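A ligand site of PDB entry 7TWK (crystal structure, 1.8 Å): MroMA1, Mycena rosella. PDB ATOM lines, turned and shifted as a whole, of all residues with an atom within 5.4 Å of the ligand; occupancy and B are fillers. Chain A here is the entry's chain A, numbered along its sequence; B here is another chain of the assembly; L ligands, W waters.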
ATOM      1  N   ILE A  19      12.445  15.503   6.147  1.00  0.00           N
ATOM      2  CA  ILE A  19      12.108  15.660   7.561  1.00  0.00           C
ATOM      3  C   ILE A  19      10.633  15.999   7.744  1.00  0.00           C
ATOM      4  O   ILE A  19       9.947  15.334   8.509  1.00  0.00           O
ATOM      5  CB  ILE A  19      13.012  16.704   8.244  1.00  0.00           C
ATOM      6  CG1 ILE A  19      14.504  16.382   8.034  1.00  0.00           C
ATOM      7  CG2 ILE A  19      12.654  16.852   9.730  1.00  0.00           C
ATOM      8  CD1 ILE A  19      14.988  15.110   8.731  1.00  0.00           C
ATOM      9  N   TYR A  99      13.937   8.142   6.621  1.00  0.00           N
ATOM     10  CA  TYR A  99      13.672   9.496   7.071  1.00  0.00           C
ATOM     11  C   TYR A  99      14.879  10.410   6.815  1.00  0.00           C
ATOM     12  O   TYR A  99      16.021  10.021   7.043  1.00  0.00           O
ATOM     13  CB  TYR A  99      13.419   9.419   8.580  1.00  0.00           C
ATOM     14  CG  TYR A  99      13.270  10.720   9.310  1.00  0.00           C
ATOM     15  CD1 TYR A  99      12.123  11.496   9.178  1.00  0.00           C
ATOM     16  CD2 TYR A  99      14.265  11.166  10.166  1.00  0.00           C
ATOM     17  CE1 TYR A  99      11.962  12.662   9.898  1.00  0.00           C
ATOM     18  CE2 TYR A  99      14.126  12.340  10.892  1.00  0.00           C
ATOM     19  CZ  TYR A  99      12.966  13.081  10.759  1.00  0.00           C
ATOM     20  OH  TYR A  99      12.809  14.234  11.482  1.00  0.00           O
ATOM     21  N   GLY A 100      14.600  11.635   6.347  1.00  0.00           N
ATOM     22  CA  GLY A 100      15.660  12.596   6.091  1.00  0.00           C
ATOM     23  C   GLY A 100      16.447  12.236   4.834  1.00  0.00           C
ATOM     24  O   GLY A 100      15.874  11.898   3.799  1.00  0.00           O
ATOM     25  N   HIS A 101      17.776  12.389   4.922  1.00  0.00           N
ATOM     26  CA  HIS A 101      18.725  11.912   3.931  1.00  0.00           C
ATOM     27  C   HIS A 101      19.125  10.494   4.352  1.00  0.00           C
ATOM     28  O   HIS A 101      19.533  10.286   5.496  1.00  0.00           O
ATOM     29  CB  HIS A 101      19.945  12.840   3.940  1.00  0.00           C
ATOM     30  CG  HIS A 101      20.972  12.563   2.891  1.00  0.00           C
ATOM     31  ND1 HIS A 101      21.532  11.305   2.704  1.00  0.00           N
ATOM     32  CD2 HIS A 101      21.602  13.404   2.030  1.00  0.00           C
ATOM     33  CE1 HIS A 101      22.433  11.369   1.730  1.00  0.00           C
ATOM     34  NE2 HIS A 101      22.508  12.657   1.310  1.00  0.00           N
ATOM     35  N   PRO A 102      19.041   9.485   3.453  1.00  0.00           N
ATOM     36  CA  PRO A 102      19.230   8.091   3.872  1.00  0.00           C
ATOM     37  C   PRO A 102      20.669   7.712   4.215  1.00  0.00           C
ATOM     38  O   PRO A 102      20.890   6.621   4.734  1.00  0.00           O
ATOM     39  CB  PRO A 102      18.800   7.303   2.633  1.00  0.00           C
ATOM     40  CG  PRO A 102      19.125   8.243   1.477  1.00  0.00           C
ATOM     41  CD  PRO A 102      18.771   9.613   2.017  1.00  0.00           C
ATOM     42  N   VAL A 104      22.750   9.984   6.029  1.00  0.00           N
ATOM     43  CA  VAL A 104      23.186  10.900   7.079  1.00  0.00           C
ATOM     44  C   VAL A 104      22.683  10.395   8.426  1.00  0.00           C
ATOM     45  O   VAL A 104      21.479  10.376   8.674  1.00  0.00           O
ATOM     46  CB  VAL A 104      22.721  12.331   6.772  1.00  0.00           C
ATOM     47  CG1 VAL A 104      22.917  13.279   7.961  1.00  0.00           C
ATOM     48  CG2 VAL A 104      23.405  12.887   5.532  1.00  0.00           C
ATOM     49  N   PHE A 105      23.611   9.960   9.285  1.00  0.00           N
ATOM     50  CA  PHE A 105      23.291   9.324  10.559  1.00  0.00           C
ATOM     51  C   PHE A 105      22.404   8.102  10.338  1.00  0.00           C
ATOM     52  O   PHE A 105      21.419   7.908  11.045  1.00  0.00           O
ATOM     53  CB  PHE A 105      22.687  10.344  11.540  1.00  0.00           C
ATOM     54  CG  PHE A 105      23.655  11.381  12.060  1.00  0.00           C
ATOM     55  CD1 PHE A 105      24.119  12.399  11.237  1.00  0.00           C
ATOM     56  CD2 PHE A 105      24.096  11.346  13.382  1.00  0.00           C
ATOM     57  CE1 PHE A 105      25.020  13.342  11.701  1.00  0.00           C
ATOM     58  CE2 PHE A 105      24.997  12.289  13.847  1.00  0.00           C
ATOM     59  CZ  PHE A 105      25.470  13.292  13.009  1.00  0.00           C
ATOM     60  N   VAL A 106      22.752   7.265   9.348  1.00  0.00           N
ATOM     61  CA  VAL A 106      22.017   6.026   9.077  1.00  0.00           C
ATOM     62  C   VAL A 106      23.021   4.909   8.810  1.00  0.00           C
ATOM     63  O   VAL A 106      23.766   4.981   7.843  1.00  0.00           O
ATOM     64  CB  VAL A 106      21.058   6.168   7.872  1.00  0.00           C
ATOM     65  CG1 VAL A 106      20.306   4.863   7.597  1.00  0.00           C
ATOM     66  CG2 VAL A 106      20.065   7.305   8.051  1.00  0.00           C
ATOM     67  N   ILE A 129      16.482  15.467   2.059  1.00  0.00           N
ATOM     68  CA  ILE A 129      16.619  16.620   2.933  1.00  0.00           C
ATOM     69  C   ILE A 129      16.979  16.146   4.340  1.00  0.00           C
ATOM     70  O   ILE A 129      16.237  15.380   4.945  1.00  0.00           O
ATOM     71  CB  ILE A 129      15.291  17.415   2.963  1.00  0.00           C
ATOM     72  CG1 ILE A 129      14.885  17.897   1.562  1.00  0.00           C
ATOM     73  CG2 ILE A 129      15.371  18.551   3.980  1.00  0.00           C
ATOM     74  CD1 ILE A 129      15.764  19.005   0.990  1.00  0.00           C
ATOM     75  N   SER A 130      18.103  16.642   4.883  1.00  0.00           N
ATOM     76  CA  SER A 130      18.542  16.204   6.211  1.00  0.00           C
ATOM     77  C   SER A 130      18.075  17.175   7.291  1.00  0.00           C
ATOM     78  O   SER A 130      17.612  18.282   6.996  1.00  0.00           O
ATOM     79  CB  SER A 130      20.047  16.090   6.254  1.00  0.00           C
ATOM     80  OG  SER A 130      20.609  17.383   6.399  1.00  0.00           O
ATOM     81  N   ALA A 131      18.240  16.775   8.558  1.00  0.00           N
ATOM     82  CA  ALA A 131      17.944  17.667   9.670  1.00  0.00           C
ATOM     83  C   ALA A 131      18.812  18.925   9.620  1.00  0.00           C
ATOM     84  O   ALA A 131      18.370  19.987  10.052  1.00  0.00           O
ATOM     85  CB  ALA A 131      18.059  16.943  11.007  1.00  0.00           C
ATOM     86  N   GLU A 132      20.044  18.814   9.103  1.00  0.00           N
ATOM     87  CA  GLU A 132      20.902  19.996   8.986  1.00  0.00           C
ATOM     88  C   GLU A 132      20.352  20.935   7.914  1.00  0.00           C
ATOM     89  O   GLU A 132      20.374  22.142   8.085  1.00  0.00           O
ATOM     90  CB  GLU A 132      22.353  19.647   8.666  1.00  0.00           C
ATOM     91  CG  GLU A 132      23.227  19.655   9.896  1.00  0.00           C
ATOM     92  CD  GLU A 132      24.687  19.307   9.650  1.00  0.00           C
ATOM     93  OE1 GLU A 132      25.156  19.453   8.488  1.00  0.00           O
ATOM     94  OE2 GLU A 132      25.358  18.878  10.617  1.00  0.00           O
ATOM     95  N   TYR A 134      17.251  21.329   7.114  1.00  0.00           N
ATOM     96  CA  TYR A 134      16.117  21.968   7.762  1.00  0.00           C
ATOM     97  C   TYR A 134      16.608  23.069   8.719  1.00  0.00           C
ATOM     98  O   TYR A 134      16.056  24.165   8.750  1.00  0.00           O
ATOM     99  CB  TYR A 134      15.275  20.905   8.471  1.00  0.00           C
ATOM    100  CG  TYR A 134      13.782  21.136   8.600  1.00  0.00           C
ATOM    101  CD1 TYR A 134      13.131  22.210   8.016  1.00  0.00           C
ATOM    102  CD2 TYR A 134      12.997  20.198   9.258  1.00  0.00           C
ATOM    103  CE1 TYR A 134      11.755  22.375   8.138  1.00  0.00           C
ATOM    104  CE2 TYR A 134      11.625  20.341   9.377  1.00  0.00           C
ATOM    105  CZ  TYR A 134      10.993  21.434   8.820  1.00  0.00           C
ATOM    106  OH  TYR A 134       9.643  21.568   8.933  1.00  0.00           O
ATOM    107  N   ILE A 171      25.559  19.507  16.779  1.00  0.00           N
ATOM    108  CA  ILE A 171      25.663  18.287  17.567  1.00  0.00           C
ATOM    109  C   ILE A 171      24.330  17.539  17.514  1.00  0.00           C
ATOM    110  O   ILE A 171      23.315  18.017  18.004  1.00  0.00           O
ATOM    111  CB  ILE A 171      26.118  18.574  19.013  1.00  0.00           C
ATOM    112  CG1 ILE A 171      27.294  19.550  19.078  1.00  0.00           C
ATOM    113  CG2 ILE A 171      26.401  17.261  19.741  1.00  0.00           C
ATOM    114  CD1 ILE A 171      27.681  19.977  20.506  1.00  0.00           C
ATOM    115  N   TRP A 172      24.368  16.328  16.946  1.00  0.00           N
ATOM    116  CA  TRP A 172      23.180  15.517  16.725  1.00  0.00           C
ATOM    117  C   TRP A 172      23.043  14.501  17.852  1.00  0.00           C
ATOM    118  O   TRP A 172      24.035  14.158  18.504  1.00  0.00           O
ATOM    119  CB  TRP A 172      23.311  14.757  15.398  1.00  0.00           C
ATOM    120  CG  TRP A 172      23.434  15.571  14.143  1.00  0.00           C
ATOM    121  CD1 TRP A 172      24.332  16.559  13.843  1.00  0.00           C
ATOM    122  CD2 TRP A 172      22.665  15.364  12.951  1.00  0.00           C
ATOM    123  NE1 TRP A 172      24.134  17.006  12.558  1.00  0.00           N
ATOM    124  CE2 TRP A 172      23.137  16.274  11.978  1.00  0.00           C
ATOM    125  CE3 TRP A 172      21.610  14.496  12.614  1.00  0.00           C
ATOM    126  CZ2 TRP A 172      22.588  16.338  10.686  1.00  0.00           C
ATOM    127  CZ3 TRP A 172      21.071  14.560  11.343  1.00  0.00           C
ATOM    128  CH2 TRP A 172      21.551  15.477  10.395  1.00  0.00           C
ATOM    129  N   GLN A 173      21.819  14.002  18.043  1.00  0.00           N
ATOM    130  CA  GLN A 173      21.504  12.883  18.937  1.00  0.00           C
ATOM    131  C   GLN A 173      21.918  13.222  20.374  1.00  0.00           C
ATOM    132  O   GLN A 173      22.436  12.352  21.085  1.00  0.00           O
ATOM    133  CB  GLN A 173      22.135  11.573  18.450  1.00  0.00           C
ATOM    134  CG  GLN A 173      21.819  11.256  16.994  1.00  0.00           C
ATOM    135  CD  GLN A 173      21.694   9.776  16.732  1.00  0.00           C
ATOM    136  OE1 GLN A 173      22.559   8.969  17.070  1.00  0.00           O
ATOM    137  NE2 GLN A 173      20.591   9.402  16.105  1.00  0.00           N
ATOM    138  N   VAL A 174      21.667  14.469  20.790  1.00  0.00           N
ATOM    139  CA  VAL A 174      22.020  14.944  22.121  1.00  0.00           C
ATOM    140  C   VAL A 174      21.133  14.248  23.149  1.00  0.00           C
ATOM    141  O   VAL A 174      21.491  14.204  24.332  1.00  0.00           O
ATOM    142  CB  VAL A 174      21.932  16.476  22.241  1.00  0.00           C
ATOM    143  CG1 VAL A 174      22.906  17.159  21.272  1.00  0.00           C
ATOM    144  CG2 VAL A 174      20.518  17.016  22.075  1.00  0.00           C
ATOM    145  N   TYR A 209      17.301  22.977  18.609  1.00  0.00           N
ATOM    146  CA  TYR A 209      16.552  22.980  17.362  1.00  0.00           C
ATOM    147  C   TYR A 209      15.757  21.687  17.201  1.00  0.00           C
ATOM    148  O   TYR A 209      16.314  20.594  17.261  1.00  0.00           O
ATOM    149  CB  TYR A 209      17.480  23.178  16.150  1.00  0.00           C
ATOM    150  CG  TYR A 209      16.771  23.021  14.820  1.00  0.00           C
ATOM    151  CD1 TYR A 209      15.745  23.881  14.453  1.00  0.00           C
ATOM    152  CD2 TYR A 209      17.086  21.975  13.959  1.00  0.00           C
ATOM    153  CE1 TYR A 209      15.052  23.723  13.259  1.00  0.00           C
ATOM    154  CE2 TYR A 209      16.415  21.808  12.759  1.00  0.00           C
ATOM    155  CZ  TYR A 209      15.402  22.683  12.407  1.00  0.00           C
ATOM    156  OH  TYR A 209      14.736  22.529  11.225  1.00  0.00           O
ATOM    157  N   ILE A 210      14.442  21.841  16.975  1.00  0.00           N
ATOM    158  CA  ILE A 210      13.586  20.761  16.504  1.00  0.00           C
ATOM    159  C   ILE A 210      12.764  21.300  15.339  1.00  0.00           C
ATOM    160  O   ILE A 210      11.903  22.163  15.522  1.00  0.00           O
ATOM    161  CB  ILE A 210      12.668  20.191  17.615  1.00  0.00           C
ATOM    162  CG1 ILE A 210      13.464  19.608  18.795  1.00  0.00           C
ATOM    163  CG2 ILE A 210      11.708  19.165  17.017  1.00  0.00           C
ATOM    164  CD1 ILE A 210      12.604  19.184  19.973  1.00  0.00           C
ATOM    165  N   GLY A 211      13.053  20.782  14.132  1.00  0.00           N
ATOM    166  CA  GLY A 211      12.280  21.154  12.953  1.00  0.00           C
ATOM    167  C   GLY A 211      10.912  20.479  12.992  1.00  0.00           C
ATOM    168  O   GLY A 211      10.784  19.376  13.531  1.00  0.00           O
ATOM    169  N   ALA A 212       9.897  21.141  12.431  1.00  0.00           N
ATOM    170  CA  ALA A 212       8.523  20.674  12.455  1.00  0.00           C
ATOM    171  C   ALA A 212       8.346  19.469  11.533  1.00  0.00           C
ATOM    172  O   ALA A 212       8.527  19.572  10.309  1.00  0.00           O
ATOM    173  CB  ALA A 212       7.602  21.818  12.066  1.00  0.00           C
ATOM    174  N   ILE A 213       7.950  18.333  12.110  1.00  0.00           N
ATOM    175  CA  ILE A 213       7.716  17.142  11.298  1.00  0.00           C
ATOM    176  C   ILE A 213       6.282  17.126  10.776  1.00  0.00           C
ATOM    177  O   ILE A 213       6.067  16.973   9.570  1.00  0.00           O
ATOM    178  CB  ILE A 213       8.107  15.848  12.051  1.00  0.00           C
ATOM    179  CG1 ILE A 213       9.611  15.814  12.368  1.00  0.00           C
ATOM    180  CG2 ILE A 213       7.695  14.619  11.246  1.00  0.00           C
ATOM    181  CD1 ILE A 213      10.005  14.777  13.410  1.00  0.00           C
ATOM    182  N   THR A 240      14.861  12.745  21.656  1.00  0.00           N
ATOM    183  CA  THR A 240      15.605  12.038  20.622  1.00  0.00           C
ATOM    184  C   THR A 240      15.499  12.739  19.265  1.00  0.00           C
ATOM    185  O   THR A 240      16.139  12.328  18.304  1.00  0.00           O
ATOM    186  CB  THR A 240      15.174  10.567  20.539  1.00  0.00           C
ATOM    187  OG1 THR A 240      13.751  10.499  20.467  1.00  0.00           O
ATOM    188  CG2 THR A 240      15.654   9.738  21.721  1.00  0.00           C
ATOM    189  N   THR A 241      14.673  13.797  19.188  1.00  0.00           N
ATOM    190  CA  THR A 241      14.537  14.605  17.981  1.00  0.00           C
ATOM    191  C   THR A 241      15.518  15.783  17.985  1.00  0.00           C
ATOM    192  O   THR A 241      15.771  16.375  16.937  1.00  0.00           O
ATOM    193  CB  THR A 241      13.109  15.144  17.835  1.00  0.00           C
ATOM    194  OG1 THR A 241      12.221  14.061  18.098  1.00  0.00           O
ATOM    195  CG2 THR A 241      12.811  15.666  16.446  1.00  0.00           C
ATOM    196  N   SER A 242      16.031  16.126  19.165  1.00  0.00           N
ATOM    197  CA  SER A 242      16.770  17.375  19.400  1.00  0.00           C
ATOM    198  C   SER A 242      18.136  17.377  18.698  1.00  0.00           C
ATOM    199  O   SER A 242      18.859  16.390  18.736  1.00  0.00           O
ATOM    200  CB  SER A 242      16.948  17.609  20.876  1.00  0.00           C
ATOM    201  OG  SER A 242      15.683  17.723  21.521  1.00  0.00           O
ATOM    202  N   THR A 243      18.478  18.522  18.107  1.00  0.00           N
ATOM    203  CA  THR A 243      19.833  18.824  17.663  1.00  0.00           C
ATOM    204  C   THR A 243      20.260  20.154  18.284  1.00  0.00           C
ATOM    205  O   THR A 243      19.439  21.051  18.450  1.00  0.00           O
ATOM    206  CB  THR A 243      19.876  18.984  16.135  1.00  0.00           C
ATOM    207  OG1 THR A 243      19.427  17.747  15.571  1.00  0.00           O
ATOM    208  CG2 THR A 243      21.261  19.298  15.613  1.00  0.00           C
ATOM    209  N   IML B 394      13.378   8.360  16.394  1.00  0.00           N
ATOM    210  CA  IML B 394      14.280   8.725  15.274  1.00  0.00           C
ATOM    211  C   IML B 394      15.735   8.343  15.526  1.00  0.00           C
ATOM    212  O   IML B 394      16.549   9.205  15.874  1.00  0.00           O
ATOM    213  CB  IML B 394      14.157  10.219  14.863  1.00  0.00           C
ATOM    214  CN  IML B 394      13.808   8.762  17.727  1.00  0.00           C
ATOM    215  CG2 IML B 394      14.769  10.420  13.475  1.00  0.00           C
ATOM    216  CG1 IML B 394      12.720  10.726  14.980  1.00  0.00           C
ATOM    217  CD1 IML B 394      12.536  12.219  14.686  1.00  0.00           C
ATOM    218  N   IML B 395      16.120   7.067  15.368  1.00  0.00           N
ATOM    219  CA  IML B 395      17.514   6.700  15.693  1.00  0.00           C
ATOM    220  C   IML B 395      18.147   5.576  14.842  1.00  0.00           C
ATOM    221  O   IML B 395      17.783   4.399  15.084  1.00  0.00           O
ATOM    222  CB  IML B 395      17.723   6.519  17.214  1.00  0.00           C
ATOM    223  CN  IML B 395      15.207   6.026  14.891  1.00  0.00           C
ATOM    224  CG2 IML B 395      16.875   5.394  17.795  1.00  0.00           C
ATOM    225  CG1 IML B 395      19.205   6.387  17.576  1.00  0.00           C
ATOM    226  CD1 IML B 395      19.613   7.198  18.777  1.00  0.00           C
ATOM    227  N   YNM B 396      18.998   5.991  13.889  1.00  0.00           N
ATOM    228  CA  YNM B 396      19.341   4.984  12.889  1.00  0.00           C
ATOM    229  C   YNM B 396      20.806   4.643  12.883  1.00  0.00           C
ATOM    230  O   YNM B 396      21.367   4.067  11.923  1.00  0.00           O
ATOM    231  CB  YNM B 396      19.039   5.430  11.470  1.00  0.00           C
ATOM    232  CG  YNM B 396      17.626   5.930  11.409  1.00  0.00           C
ATOM    233  CD1 YNM B 396      17.378   7.291  11.523  1.00  0.00           C
ATOM    234  CD2 YNM B 396      16.600   5.021  11.215  1.00  0.00           C
ATOM    235  CE1 YNM B 396      16.068   7.760  11.473  1.00  0.00           C
ATOM    236  CE2 YNM B 396      15.290   5.481  11.159  1.00  0.00           C
ATOM    237  OH  YNM B 396      13.728   7.287  11.224  1.00  0.00           O
ATOM    238  CZ  YNM B 396      15.024   6.855  11.291  1.00  0.00           C
ATOM    239  CM  YNM B 396      19.664   7.314  13.830  1.00  0.00           C
HETATM  240  N1  LIG L   1      18.687  10.581   8.124  1.00  0.00           N
HETATM  241  C1  LIG L   1      18.294  11.581   9.136  1.00  0.00           C
HETATM  242  C2  LIG L   1      19.085  11.365  10.425  1.00  0.00           C
HETATM  243  C3  LIG L   1      18.229  11.129  11.623  1.00  0.00           C
HETATM  244  S1  LIG L   1      19.189  10.577  13.039  1.00  0.00           S
HETATM  245  C4  LIG L   1      18.590  12.986   8.600  1.00  0.00           C
HETATM  246  O1  LIG L   1      18.417  13.980   9.315  1.00  0.00           O
HETATM  247  O2  LIG L   1      19.010  13.154   7.441  1.00  0.00           O
HETATM  248  C5  LIG L   1      18.301  11.442  14.351  1.00  0.00           C
HETATM  249  C6  LIG L   1      18.925  12.759  14.724  1.00  0.00           C
HETATM  250  O3  LIG L   1      18.724  13.706  13.655  1.00  0.00           O
HETATM  251  C7  LIG L   1      18.287  13.422  15.944  1.00  0.00           C
HETATM  252  O4  LIG L   1      18.806  12.904  17.173  1.00  0.00           O
HETATM  253  C8  LIG L   1      18.632  14.882  15.702  1.00  0.00           C
HETATM  254  O5  LIG L   1      19.973  15.168  16.050  1.00  0.00           O
HETATM  255  C9  LIG L   1      18.393  14.976  14.186  1.00  0.00           C
HETATM  256  N2  LIG L   1      17.004  15.279  13.832  1.00  0.00           N
HETATM  257  C10 LIG L   1      16.083  14.427  13.277  1.00  0.00           C
HETATM  258  N3  LIG L   1      14.905  14.978  13.091  1.00  0.00           N
HETATM  259  C11 LIG L   1      15.061  16.274  13.539  1.00  0.00           C
HETATM  260  C12 LIG L   1      14.174  17.365  13.600  1.00  0.00           C
HETATM  261  N4  LIG L   1      12.903  17.310  13.218  1.00  0.00           N
HETATM  262  N5  LIG L   1      14.654  18.527  14.112  1.00  0.00           N
HETATM  263  C13 LIG L   1      15.934  18.582  14.514  1.00  0.00           C
HETATM  264  N6  LIG L   1      16.861  17.627  14.499  1.00  0.00           N
HETATM  265  C14 LIG L   1      16.355  16.486  13.990  1.00  0.00           C
HETATM  266  O   HOH W   1      18.104  10.157  17.836  1.00  0.00           O
HETATM  267  O   HOH W   2      18.534  14.017  20.244  1.00  0.00           O
HETATM  268  O   HOH W   3      18.912  11.213  20.132  1.00  0.00           O
HETATM  269  O   HOH W   4      16.996   8.360   8.682  1.00  0.00           O
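OG1 of Thr 243 lies within hydrogen-bond range of O5 of the ligand (2.7 Å).
The backbone carbonyl oxygen (O) of Tyr 99 sits at hydrogen-bond distance from a nitrogen (N1) of the ligand (2.9 Å).
A nitrogen (N3) of the ligand is in hydrogen-bond range of the side-chain hydroxyl (OH) of Tyr 99.
The backbone NH (N) of Gly 211 sits at hydrogen-bond distance from a nitrogen (N5) of the ligand (2.8 Å).
A nitrogen (N4) of the ligand sits at hydrogen-bond distance from the backbone carbonyl oxygen (O) of Gly 211 (3.0 Å).
N of His 101 lies within hydrogen-bond range of O2 of the ligand, at 2.9 Å.
The backbone carbonyl oxygen of His 101 is in hydrogen-bond range of a nitrogen (N1) of the ligand (2.8 Å).
A nitrogen (N1) of the ligand is in hydrogen-bond range of the backbone carbonyl oxygen (O) of Val 104.
The backbone NH (N) of Ala 131 is in hydrogen-bond range of an oxygen (O1) of the ligand.
O of Thr 240 sits at hydrogen-bond distance from O4 of the ligand, at 3.0 Å.
N of Gln 173 sits at hydrogen-bond distance from O5 of the ligand (3.0 Å).
The side-chain amide nitrogen (NE2) of Gln 173 sits close to a sulfur (S1) of the ligand, at 3.6 Å.
An oxygen (O5) of the ligand sits at hydrogen-bond distance from the backbone carbonyl oxygen of Ser 242 (3.2 Å).
N of Tyr 209 lies within hydrogen-bond range of O of Thr 243 (2.9 Å).
O of Ile 129 sits at hydrogen-bond distance from N of His 101, at 3.4 Å.
The side-chain carboxylate of Glu 132 lies within hydrogen-bond range of the indole nitrogen of Trp 172, 3.0 Å away.
OG of Ser 130 is in hydrogen-bond range of N of Glu 132, at 3.1 Å.
OH of Tyr 209 lies close to O of Tyr 134, at 3.2 Å.
A nitrogen (N6) of the ligand sits close to the backbone carbonyl oxygen of Thr 241, 2.9 Å away.
Ile 19 touches the ligand (CG2 to N4, 3.5 Å).
CA of Gly 100 touches O2 of the ligand, at 3.7 Å.
Phe 105 touches the ligand.
CG2 of Val 106 touches N1 of the ligand, at 3.6 Å.
CA of Ser 130 touches O2 of the ligand (3.3 Å).
Trp 172 touches the ligand.
O of Tyr 209 touches C13 of the ligand, at 3.4 Å.
Ile 210 touches the ligand.
Ile 213 touches the ligand (CG1 to N4, 3.7 Å).
IML 394 of chain B touches the ligand (O to C5, 3.2 Å).
CM of YNM 396 of chain B touches S1 of the ligand, 3.4 Å away.
Within 4 Å of the ligand: Ile 19, Tyr 99, Gly 100, His 101, Val 104, Phe 105, Val 106, Ser 130, Ala 131, Trp 172, Gln 173, Tyr 209, Ile 210, Gly 211, Ile 213, Thr 240, Thr 241, Ser 242, Thr 243, IML 394 of chain B and YNM 396 of chain B.
Water W4 bridges the backbone carbonyl oxygen of Tyr 99 (2.5 Å) and a nitrogen (N1) of the ligand (2.8 Å).
Water W1 lies within hydrogen-bond range of O of IML 394 of chain B (2.7 Å), an oxygen (O4) of the ligand (2.9 Å), the backbone carbonyl oxygen of Thr 240 (3.0 Å) and the side-chain amide nitrogen of Gln 173 (3.1 Å).
Water W2 lies within hydrogen-bond range of O of Ser 242 (2.8 Å), N of Val 174 (3.2 Å) and O4 of the ligand (3.3 Å).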
